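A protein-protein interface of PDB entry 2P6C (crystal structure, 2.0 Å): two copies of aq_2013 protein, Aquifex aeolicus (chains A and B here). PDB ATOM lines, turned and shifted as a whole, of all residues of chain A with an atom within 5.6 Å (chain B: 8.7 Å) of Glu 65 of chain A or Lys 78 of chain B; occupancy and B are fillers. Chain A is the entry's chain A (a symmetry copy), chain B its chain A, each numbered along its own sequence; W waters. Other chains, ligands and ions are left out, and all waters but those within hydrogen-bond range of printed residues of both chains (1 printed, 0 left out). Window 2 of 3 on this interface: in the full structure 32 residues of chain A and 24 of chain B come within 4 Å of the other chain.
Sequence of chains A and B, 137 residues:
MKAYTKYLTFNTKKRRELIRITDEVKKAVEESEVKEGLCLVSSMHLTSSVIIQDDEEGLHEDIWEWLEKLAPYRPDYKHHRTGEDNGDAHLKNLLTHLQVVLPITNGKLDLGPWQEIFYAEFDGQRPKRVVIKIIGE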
ATOM      1  N   GLU A  56     -13.087  18.124 -17.938  1.00  0.00           N
ATOM      2  CA  GLU A  56     -13.773  17.199 -17.016  1.00  0.00           C
ATOM      3  C   GLU A  56     -15.283  17.016 -17.304  1.00  0.00           C
ATOM      4  O   GLU A  56     -16.047  17.969 -17.386  1.00  0.00           O
ATOM      5  CB  GLU A  56     -13.572  17.721 -15.593  1.00  0.00           C
ATOM      6  CG  GLU A  56     -13.530  16.593 -14.563  1.00  0.00           C
ATOM      7  CD  GLU A  56     -14.923  16.358 -14.032  1.00  0.00           C
ATOM      8  OE1 GLU A  56     -15.537  17.303 -13.557  1.00  0.00           O
ATOM      9  OE2 GLU A  56     -15.387  15.219 -14.094  1.00  0.00           O
ATOM     10  N   GLY A  58     -17.791  15.613 -15.488  1.00  0.00           N
ATOM     11  CA  GLY A  58     -18.735  16.029 -14.474  1.00  0.00           C
ATOM     12  C   GLY A  58     -19.017  17.514 -14.621  1.00  0.00           C
ATOM     13  O   GLY A  58     -20.158  17.958 -14.466  1.00  0.00           O
ATOM     14  N   LEU A  59     -17.980  18.291 -14.934  1.00  0.00           N
ATOM     15  CA  LEU A  59     -18.160  19.724 -15.058  1.00  0.00           C
ATOM     16  C   LEU A  59     -19.006  20.036 -16.287  1.00  0.00           C
ATOM     17  O   LEU A  59     -19.783  20.981 -16.314  1.00  0.00           O
ATOM     18  CB  LEU A  59     -16.776  20.371 -15.189  1.00  0.00           C
ATOM     19  CG  LEU A  59     -16.252  20.939 -13.862  1.00  0.00           C
ATOM     20  CD1 LEU A  59     -14.925  21.682 -14.030  1.00  0.00           C
ATOM     21  CD2 LEU A  59     -17.220  21.933 -13.219  1.00  0.00           C
ATOM     22  N   HIS A  60     -18.850  19.231 -17.326  1.00  0.00           N
ATOM     23  CA  HIS A  60     -19.651  19.448 -18.511  1.00  0.00           C
ATOM     24  C   HIS A  60     -21.101  19.226 -18.148  1.00  0.00           C
ATOM     25  O   HIS A  60     -21.980  19.956 -18.599  1.00  0.00           O
ATOM     26  CB  HIS A  60     -19.232  18.500 -19.619  1.00  0.00           C
ATOM     27  CG  HIS A  60     -17.852  18.760 -20.134  1.00  0.00           C
ATOM     28  ND1 HIS A  60     -17.258  17.975 -21.095  1.00  0.00           N
ATOM     29  CD2 HIS A  60     -16.946  19.715 -19.814  1.00  0.00           C
ATOM     30  CE1 HIS A  60     -16.044  18.432 -21.345  1.00  0.00           C
ATOM     31  NE2 HIS A  60     -15.830  19.486 -20.580  1.00  0.00           N
ATOM     32  N   GLU A  61     -21.357  18.215 -17.328  1.00  0.00           N
ATOM     33  CA  GLU A  61     -22.741  17.980 -16.956  1.00  0.00           C
ATOM     34  C   GLU A  61     -23.243  19.104 -16.061  1.00  0.00           C
ATOM     35  O   GLU A  61     -24.357  19.592 -16.198  1.00  0.00           O
ATOM     36  CB  GLU A  61     -22.835  16.642 -16.216  1.00  0.00           C
ATOM     37  CG  GLU A  61     -24.192  16.452 -15.528  1.00  0.00           C
ATOM     38  CD  GLU A  61     -24.508  14.976 -15.404  1.00  0.00           C
ATOM     39  OE1 GLU A  61     -23.615  14.165 -15.634  1.00  0.00           O
ATOM     40  OE2 GLU A  61     -25.640  14.644 -15.070  1.00  0.00           O
ATOM     41  N   ASP A  62     -22.412  19.575 -15.134  1.00  0.00           N
ATOM     42  CA  ASP A  62     -22.826  20.670 -14.256  1.00  0.00           C
ATOM     43  C   ASP A  62     -23.215  21.918 -15.056  1.00  0.00           C
ATOM     44  O   ASP A  62     -24.134  22.641 -14.714  1.00  0.00           O
ATOM     45  CB  ASP A  62     -21.696  21.025 -13.270  1.00  0.00           C
ATOM     46  CG  ASP A  62     -21.416  19.890 -12.283  1.00  0.00           C
ATOM     47  OD1 ASP A  62     -22.373  19.253 -11.829  1.00  0.00           O
ATOM     48  OD2 ASP A  62     -20.248  19.685 -11.951  1.00  0.00           O
ATOM     49  N   ILE A  63     -22.474  22.203 -16.141  1.00  0.00           N
ATOM     50  CA  ILE A  63     -22.763  23.472 -16.872  1.00  0.00           C
ATOM     51  C   ILE A  63     -24.128  23.336 -17.599  1.00  0.00           C
ATOM     52  O   ILE A  63     -24.895  24.283 -17.716  1.00  0.00           O
ATOM     53  CB  ILE A  63     -21.581  23.996 -17.765  1.00  0.00           C
ATOM     54  CG1 ILE A  63     -21.055  22.940 -18.750  1.00  0.00           C
ATOM     55  CG2 ILE A  63     -20.357  24.428 -16.894  1.00  0.00           C
ATOM     56  CD1 ILE A  63     -20.547  23.521 -20.071  1.00  0.00           C
ATOM     57  N   TRP A  64     -24.412  22.165 -18.163  1.00  0.00           N
ATOM     58  CA  TRP A  64     -25.719  22.066 -18.782  1.00  0.00           C
ATOM     59  C   TRP A  64     -26.832  22.232 -17.744  1.00  0.00           C
ATOM     60  O   TRP A  64     -27.808  22.935 -17.976  1.00  0.00           O
ATOM     61  CB  TRP A  64     -25.840  20.724 -19.484  1.00  0.00           C
ATOM     62  CG  TRP A  64     -25.010  20.717 -20.713  1.00  0.00           C
ATOM     63  CD1 TRP A  64     -23.842  19.970 -20.926  1.00  0.00           C
ATOM     64  CD2 TRP A  64     -25.226  21.494 -21.914  1.00  0.00           C
ATOM     65  NE1 TRP A  64     -23.293  20.194 -22.146  1.00  0.00           N
ATOM     66  CE2 TRP A  64     -24.160  21.175 -22.804  1.00  0.00           C
ATOM     67  CE3 TRP A  64     -26.179  22.403 -22.305  1.00  0.00           C
ATOM     68  CZ2 TRP A  64     -24.088  21.762 -24.051  1.00  0.00           C
ATOM     69  CZ3 TRP A  64     -26.105  22.993 -23.557  1.00  0.00           C
ATOM     70  CH2 TRP A  64     -25.049  22.672 -24.432  1.00  0.00           C
ATOM     71  N   GLU A  65     -26.674  21.587 -16.590  1.00  0.00           N
ATOM     72  CA  GLU A  65     -27.686  21.678 -15.544  1.00  0.00           C
ATOM     73  C   GLU A  65     -27.833  23.143 -15.042  1.00  0.00           C
ATOM     74  O   GLU A  65     -28.929  23.656 -14.855  1.00  0.00           O
ATOM     75  CB  GLU A  65     -27.323  20.663 -14.414  1.00  0.00           C
ATOM     76  CG  GLU A  65     -27.325  19.181 -14.897  1.00  0.00           C
ATOM     77  CD  GLU A  65     -26.995  18.168 -13.779  1.00  0.00           C
ATOM     78  OE1 GLU A  65     -26.335  18.549 -12.821  1.00  0.00           O
ATOM     79  OE2 GLU A  65     -27.418  17.018 -13.888  1.00  0.00           O
ATOM     80  N   TRP A  66     -26.684  23.880 -14.846  1.00  0.00           N
ATOM     81  CA  TRP A  66     -26.684  25.293 -14.414  1.00  0.00           C
ATOM     82  C   TRP A  66     -27.317  26.216 -15.469  1.00  0.00           C
ATOM     83  O   TRP A  66     -28.141  27.080 -15.185  1.00  0.00           O
ATOM     84  CB  TRP A  66     -25.227  25.707 -14.186  1.00  0.00           C
ATOM     85  CG  TRP A  66     -25.080  27.118 -13.743  1.00  0.00           C
ATOM     86  CD1 TRP A  66     -25.412  27.637 -12.481  1.00  0.00           C
ATOM     87  CD2 TRP A  66     -24.427  28.190 -14.468  1.00  0.00           C
ATOM     88  NE1 TRP A  66     -25.043  28.936 -12.334  1.00  0.00           N
ATOM     89  CE2 TRP A  66     -24.411  29.319 -13.599  1.00  0.00           C
ATOM     90  CE3 TRP A  66     -23.886  28.300 -15.730  1.00  0.00           C
ATOM     91  CZ2 TRP A  66     -23.853  30.511 -14.017  1.00  0.00           C
ATOM     92  CZ3 TRP A  66     -23.327  29.498 -16.146  1.00  0.00           C
ATOM     93  CH2 TRP A  66     -23.316  30.609 -15.282  1.00  0.00           C
ATOM     94  N   LEU A  67     -26.890  26.005 -16.738  1.00  0.00           N
ATOM     95  CA  LEU A  67     -27.531  26.712 -17.857  1.00  0.00           C
ATOM     96  C   LEU A  67     -29.076  26.523 -17.878  1.00  0.00           C
ATOM     97  O   LEU A  67     -29.842  27.469 -18.007  1.00  0.00           O
ATOM     98  CB  LEU A  67     -26.893  26.217 -19.172  1.00  0.00           C
ATOM     99  CG  LEU A  67     -25.445  26.714 -19.401  1.00  0.00           C
ATOM    100  CD1 LEU A  67     -24.902  26.319 -20.775  1.00  0.00           C
ATOM    101  CD2 LEU A  67     -25.321  28.236 -19.313  1.00  0.00           C
ATOM    102  N   GLU A  68     -29.519  25.280 -17.772  1.00  0.00           N
ATOM    103  CA  GLU A  68     -30.950  25.020 -17.832  1.00  0.00           C
ATOM    104  C   GLU A  68     -31.630  25.693 -16.633  1.00  0.00           C
ATOM    105  O   GLU A  68     -32.751  26.215 -16.732  1.00  0.00           O
ATOM    106  CB  GLU A  68     -31.189  23.519 -17.809  1.00  0.00           C
ATOM    107  CG  GLU A  68     -32.517  23.122 -18.418  1.00  0.00           C
ATOM    108  CD  GLU A  68     -32.735  23.712 -19.803  1.00  0.00           C
ATOM    109  OE1 GLU A  68     -31.756  24.158 -20.445  1.00  0.00           O
ATOM    110  OE2 GLU A  68     -33.898  23.711 -20.261  1.00  0.00           O
ATOM    111  N   LYS A  69     -30.928  25.664 -15.502  1.00  0.00           N
ATOM    112  CA  LYS A  69     -31.424  26.266 -14.273  1.00  0.00           C
ATOM    113  C   LYS A  69     -31.537  27.789 -14.398  1.00  0.00           C
ATOM    114  O   LYS A  69     -32.510  28.403 -13.981  1.00  0.00           O
ATOM    115  CB  LYS A  69     -30.453  25.903 -13.152  1.00  0.00           C
ATOM    116  CG  LYS A  69     -30.389  26.984 -12.077  1.00  0.00           C
ATOM    117  CD  LYS A  69     -31.566  26.887 -11.107  1.00  0.00           C
ATOM    118  CE  LYS A  69     -31.117  26.659  -9.665  1.00  0.00           C
ATOM    119  NZ  LYS A  69     -32.285  26.635  -8.794  1.00  0.00           N
ATOM    120  N   LEU A  70     -30.479  28.431 -14.977  1.00  0.00           N
ATOM    121  CA  LEU A  70     -30.458  29.913 -15.095  1.00  0.00           C
ATOM    122  C   LEU A  70     -31.209  30.401 -16.340  1.00  0.00           C
ATOM    123  O   LEU A  70     -31.853  31.442 -16.338  1.00  0.00           O
ATOM    124  CB  LEU A  70     -29.007  30.486 -15.158  1.00  0.00           C
ATOM    125  CG  LEU A  70     -28.137  30.270 -13.905  1.00  0.00           C
ATOM    126  CD1 LEU A  70     -26.830  31.084 -13.921  1.00  0.00           C
ATOM    127  CD2 LEU A  70     -28.829  30.611 -12.585  1.00  0.00           C
ATOM    128  N   ARG B  74     -21.678  23.942  -3.727  1.00  0.00           N
ATOM    129  CA  ARG B  74     -22.562  22.820  -3.583  1.00  0.00           C
ATOM    130  C   ARG B  74     -21.714  21.606  -3.362  1.00  0.00           C
ATOM    131  O   ARG B  74     -20.724  21.390  -4.048  1.00  0.00           O
ATOM    132  CB  ARG B  74     -23.360  22.649  -4.879  1.00  0.00           C
ATOM    133  CG  ARG B  74     -24.604  23.531  -4.938  1.00  0.00           C
ATOM    134  CD  ARG B  74     -25.791  22.814  -5.593  1.00  0.00           C
ATOM    135  NE  ARG B  74     -26.068  21.569  -4.878  1.00  0.00           N
ATOM    136  CZ  ARG B  74     -27.311  21.392  -4.403  1.00  0.00           C
ATOM    137  NH1 ARG B  74     -28.250  22.291  -4.648  1.00  0.00           N
ATOM    138  NH2 ARG B  74     -27.560  20.373  -3.570  1.00  0.00           N
ATOM    139  N   PRO B  75     -22.104  20.695  -2.530  1.00  0.00           N
ATOM    140  CA  PRO B  75     -21.382  19.467  -2.273  1.00  0.00           C
ATOM    141  C   PRO B  75     -21.600  18.314  -3.312  1.00  0.00           C
ATOM    142  O   PRO B  75     -20.818  17.400  -3.485  1.00  0.00           O
ATOM    143  CB  PRO B  75     -21.843  18.971  -0.910  1.00  0.00           C
ATOM    144  CG  PRO B  75     -23.299  19.390  -0.811  1.00  0.00           C
ATOM    145  CD  PRO B  75     -23.233  20.791  -1.584  1.00  0.00           C
ATOM    146  N   ASP B  76     -22.748  18.474  -4.017  1.00  0.00           N
ATOM    147  CA  ASP B  76     -23.217  17.448  -4.949  1.00  0.00           C
ATOM    148  C   ASP B  76     -22.938  17.728  -6.469  1.00  0.00           C
ATOM    149  O   ASP B  76     -23.491  17.127  -7.344  1.00  0.00           O
ATOM    150  CB  ASP B  76     -24.742  17.166  -4.707  1.00  0.00           C
ATOM    151  CG  ASP B  76     -25.592  18.446  -4.700  1.00  0.00           C
ATOM    152  OD1 ASP B  76     -25.025  19.503  -4.983  1.00  0.00           O
ATOM    153  OD2 ASP B  76     -26.806  18.368  -4.439  1.00  0.00           O
ATOM    154  N   TYR B  77     -22.071  18.724  -6.786  1.00  0.00           N
ATOM    155  CA  TYR B  77     -21.837  18.931  -8.230  1.00  0.00           C
ATOM    156  C   TYR B  77     -21.184  17.666  -8.755  1.00  0.00           C
ATOM    157  O   TYR B  77     -20.450  16.997  -8.031  1.00  0.00           O
ATOM    158  CB  TYR B  77     -20.864  20.125  -8.453  1.00  0.00           C
ATOM    159  CG  TYR B  77     -21.520  21.478  -8.325  1.00  0.00           C
ATOM    160  CD1 TYR B  77     -22.647  21.799  -9.073  1.00  0.00           C
ATOM    161  CD2 TYR B  77     -20.996  22.439  -7.448  1.00  0.00           C
ATOM    162  CE1 TYR B  77     -23.259  23.040  -8.943  1.00  0.00           C
ATOM    163  CE2 TYR B  77     -21.609  23.682  -7.318  1.00  0.00           C
ATOM    164  CZ  TYR B  77     -22.735  23.980  -8.059  1.00  0.00           C
ATOM    165  OH  TYR B  77     -23.384  25.183  -7.898  1.00  0.00           O
ATOM    166  N   LYS B  78     -21.460  17.330 -10.009  1.00  0.00           N
ATOM    167  CA  LYS B  78     -20.908  16.124 -10.602  1.00  0.00           C
ATOM    168  C   LYS B  78     -19.390  16.193 -10.672  1.00  0.00           C
ATOM    169  O   LYS B  78     -18.706  15.168 -10.620  1.00  0.00           O
ATOM    170  CB  LYS B  78     -21.490  15.912 -12.001  1.00  0.00           C
ATOM    171  CG  LYS B  78     -23.007  15.766 -12.020  1.00  0.00           C
ATOM    172  CD  LYS B  78     -23.475  14.680 -11.068  1.00  0.00           C
ATOM    173  CE  LYS B  78     -24.955  14.397 -11.258  1.00  0.00           C
ATOM    174  NZ  LYS B  78     -25.764  15.647 -11.118  1.00  0.00           N
ATOM    175  N   HIS B  79     -18.868  17.410 -10.782  1.00  0.00           N
ATOM    176  CA  HIS B  79     -17.414  17.626 -10.846  1.00  0.00           C
ATOM    177  C   HIS B  79     -16.732  16.985  -9.630  1.00  0.00           C
ATOM    178  O   HIS B  79     -15.562  16.636  -9.647  1.00  0.00           O
ATOM    179  CB  HIS B  79     -17.131  19.140 -10.884  1.00  0.00           C
ATOM    180  CG  HIS B  79     -15.638  19.409 -10.974  1.00  0.00           C
ATOM    181  ND1 HIS B  79     -14.837  18.887 -11.941  1.00  0.00           N
ATOM    182  CD2 HIS B  79     -14.853  20.246 -10.155  1.00  0.00           C
ATOM    183  CE1 HIS B  79     -13.604  19.390 -11.693  1.00  0.00           C
ATOM    184  NE2 HIS B  79     -13.584  20.205 -10.631  1.00  0.00           N
ATOM    185  N   HIS B  80     -17.522  16.854  -8.546  1.00  0.00           N
ATOM    186  CA  HIS B  80     -16.996  16.296  -7.292  1.00  0.00           C
ATOM    187  C   HIS B  80     -16.632  14.815  -7.388  1.00  0.00           C
ATOM    188  O   HIS B  80     -16.104  14.216  -6.456  1.00  0.00           O
ATOM    189  CB  HIS B  80     -18.069  16.491  -6.216  1.00  0.00           C
ATOM    190  CG  HIS B  80     -17.629  15.871  -4.903  1.00  0.00           C
ATOM    191  ND1 HIS B  80     -18.256  14.802  -4.347  1.00  0.00           N
ATOM    192  CD2 HIS B  80     -16.656  16.336  -4.001  1.00  0.00           C
ATOM    193  CE1 HIS B  80     -17.657  14.622  -3.148  1.00  0.00           C
ATOM    194  NE2 HIS B  80     -16.698  15.524  -2.912  1.00  0.00           N
ATOM    195  N   ARG B  81     -16.987  14.200  -8.527  1.00  0.00           N
ATOM    196  CA  ARG B  81     -16.587  12.833  -8.730  1.00  0.00           C
ATOM    197  C   ARG B  81     -15.073  12.739  -8.662  1.00  0.00           C
ATOM    198  O   ARG B  81     -14.499  11.692  -8.392  1.00  0.00           O
ATOM    199  CB  ARG B  81     -17.104  12.364 -10.100  1.00  0.00           C
ATOM    200  CG  ARG B  81     -16.295  12.928 -11.275  1.00  0.00           C
ATOM    201  CD  ARG B  81     -17.021  12.781 -12.622  1.00  0.00           C
ATOM    202  NE  ARG B  81     -17.464  11.399 -12.833  1.00  0.00           N
ATOM    203  CZ  ARG B  81     -16.625  10.549 -13.459  1.00  0.00           C
ATOM    204  NH1 ARG B  81     -15.448  10.972 -13.883  1.00  0.00           N
ATOM    205  NH2 ARG B  81     -16.951   9.257 -13.564  1.00  0.00           N
ATOM    206  N   THR B  82     -14.418  13.858  -8.940  1.00  0.00           N
ATOM    207  CA  THR B  82     -12.965  13.846  -8.914  1.00  0.00           C
ATOM    208  C   THR B  82     -12.433  14.098  -7.505  1.00  0.00           C
ATOM    209  O   THR B  82     -11.232  14.132  -7.268  1.00  0.00           O
ATOM    210  CB  THR B  82     -12.465  14.927  -9.879  1.00  0.00           C
ATOM    211  OG1 THR B  82     -12.861  16.209  -9.389  1.00  0.00           O
ATOM    212  CG2 THR B  82     -13.072  14.722 -11.271  1.00  0.00           C
ATOM    213  N   GLY B  83     -13.354  14.299  -6.536  1.00  0.00           N
ATOM    214  CA  GLY B  83     -12.935  14.710  -5.189  1.00  0.00           C
ATOM    215  C   GLY B  83     -12.681  16.222  -5.079  1.00  0.00           C
ATOM    216  O   GLY B  83     -12.323  16.756  -4.030  1.00  0.00           O
ATOM    217  N   GLU B  84     -12.835  16.920  -6.216  1.00  0.00           N
ATOM    218  CA  GLU B  84     -12.666  18.394  -6.222  1.00  0.00           C
ATOM    219  C   GLU B  84     -14.026  18.977  -5.988  1.00  0.00           C
ATOM    220  O   GLU B  84     -14.998  18.633  -6.647  1.00  0.00           O
ATOM    221  CB  GLU B  84     -12.044  19.023  -7.543  1.00  0.00           C
ATOM    222  CG  GLU B  84     -10.822  18.260  -8.049  1.00  0.00           C
ATOM    223  CD  GLU B  84      -9.700  19.246  -8.269  1.00  0.00           C
ATOM    224  OE1 GLU B  84      -9.768  20.003  -9.224  1.00  0.00           O
ATOM    225  OE2 GLU B  84      -8.806  19.311  -7.422  1.00  0.00           O
ATOM    226  N   ASP B  85     -14.147  19.893  -5.041  1.00  0.00           N
ATOM    227  CA  ASP B  85     -15.468  20.475  -4.896  1.00  0.00           C
ATOM    228  C   ASP B  85     -15.424  21.988  -5.045  1.00  0.00           C
ATOM    229  O   ASP B  85     -15.966  22.732  -4.238  1.00  0.00           O
ATOM    230  CB  ASP B  85     -16.029  20.090  -3.523  1.00  0.00           C
ATOM    231  CG  ASP B  85     -15.160  20.657  -2.400  1.00  0.00           C
ATOM    232  OD1 ASP B  85     -14.156  21.308  -2.701  1.00  0.00           O
ATOM    233  OD2 ASP B  85     -15.508  20.455  -1.240  1.00  0.00           O
ATOM    234  N   GLY B  87     -16.518  23.149  -7.946  1.00  0.00           N
ATOM    235  CA  GLY B  87     -17.442  23.304  -9.056  1.00  0.00           C
ATOM    236  C   GLY B  87     -18.016  24.708  -9.152  1.00  0.00           C
ATOM    237  O   GLY B  87     -18.079  25.280 -10.239  1.00  0.00           O
ATOM    238  N   LEU B  91     -18.298  27.669 -12.334  1.00  0.00           N
ATOM    239  CA  LEU B  91     -19.521  28.335 -12.749  1.00  0.00           C
ATOM    240  C   LEU B  91     -19.357  29.851 -12.625  1.00  0.00           C
ATOM    241  O   LEU B  91     -19.777  30.603 -13.514  1.00  0.00           O
ATOM    242  CB  LEU B  91     -20.701  27.830 -11.911  1.00  0.00           C
ATOM    243  CG  LEU B  91     -20.993  26.330 -12.064  1.00  0.00           C
ATOM    244  CD1 LEU B  91     -22.137  25.926 -11.134  1.00  0.00           C
ATOM    245  CD2 LEU B  91     -21.342  26.004 -13.518  1.00  0.00           C
HETATM  246  O   HOH W   1     -13.988  13.083 -14.333  1.00  0.00           O
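The backbone NH (N) of Lys 78 of chain B sits at hydrogen-bond distance from the side-chain carboxylate (OD1) of Asp 62 of chain A (2.8 Å). NZ of Lys 78 of chain B is in salt-bridge range of OE1 of Glu 65 of chain A, at 3.4 Å. N of His 79 of chain B sits at hydrogen-bond distance from OD2 of Asp 62 of chain A (2.9 Å). A ring nitrogen (ND1) of His 79 of chain B lies close to the side-chain carboxylate of Glu 56 of chain A (2.4 Å).
The backbone carbonyl oxygen (O) of His 79 of chain B is in hydrogen-bond range of the side-chain hydroxyl (OG1) of Thr 82 of chain B, at 2.7 Å. OG1 of Thr 82 of chain B lies close to N of Glu 84 of chain B (3.3 Å). OE2 of Glu 56 of chain A lies within hydrogen-bond range of N of Gly 58 of chain A, 2.8 Å away. OE1 of Glu 56 of chain A sits at hydrogen-bond distance from N of Leu 59 of chain A (3.0 Å).
Among the printed residues, merely in contact across the chains: Glu 56 of chain A with Arg 81 of chain B (3.3 Å), Glu 56 of chain A with Thr 82 of chain B (3.7 Å), Gly 58 of chain A with Lys 78 of chain B (3.5 Å), Gly 58 of chain A with His 79 of chain B (3.8 Å), Leu 59 of chain A with His 79 of chain B (3.1 Å), Glu 61 of chain A with Lys 78 of chain B (3.8 Å), Asp 62 of chain A with Tyr 77 of chain B (3.6 Å), Ile 63 of chain A with Leu 91 of chain B (3.9 Å) and Trp 66 of chain A with Leu 91 of chain B (3.9 Å).
Printed residues of chain B within 4 Å of Glu 56 of chain A: His 79, Arg 81 and Thr 82. Of the printed residues of chain B, Gly 58 of chain A touches Lys 78 (3.5 Å) and His 79 (3.8 Å). Of the printed residues of chain B, Leu 59 of chain A touches His 79 (3.1 Å). Glu 65 of chain A touches one residue of chain B. Pro 75 of chain B touches none of the printed residues of chain A. Printed residues of chain A within 4 Å of Tyr 77 of chain B: Asp 62. Of chain A, only Gly 58, Glu 61, Asp 62 and Glu 65 come within 4 Å of Lys 78 of chain B. The nearest residue of chain B that does not touch Glu 65 of chain A is Tyr 77 of chain B (6.2 Å).
Printed residues of chain A that touch a printed residue of chain B: Glu 56, Gly 58, Leu 59, Glu 61, Asp 62, Ile 63, Glu 65 and Trp 66. Hydrophobic or aromatic side chains of chain A that line the printed part of chain B: Leu 59, Ile 63 and Trp 66. Along chain A the printed residues that touch a printed residue of chain B span positions 56 to 66. Hydrophobic or aromatic side chains of chain B within 4 Å of the printed part of chain A: Tyr 77, His 79 and Leu 91.
No position is printed for both chains.
Water W1 bridges OE2 of Glu 56 of chain A (2.6 Å) and NH1 of Arg 81 of chain B (2.6 Å).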
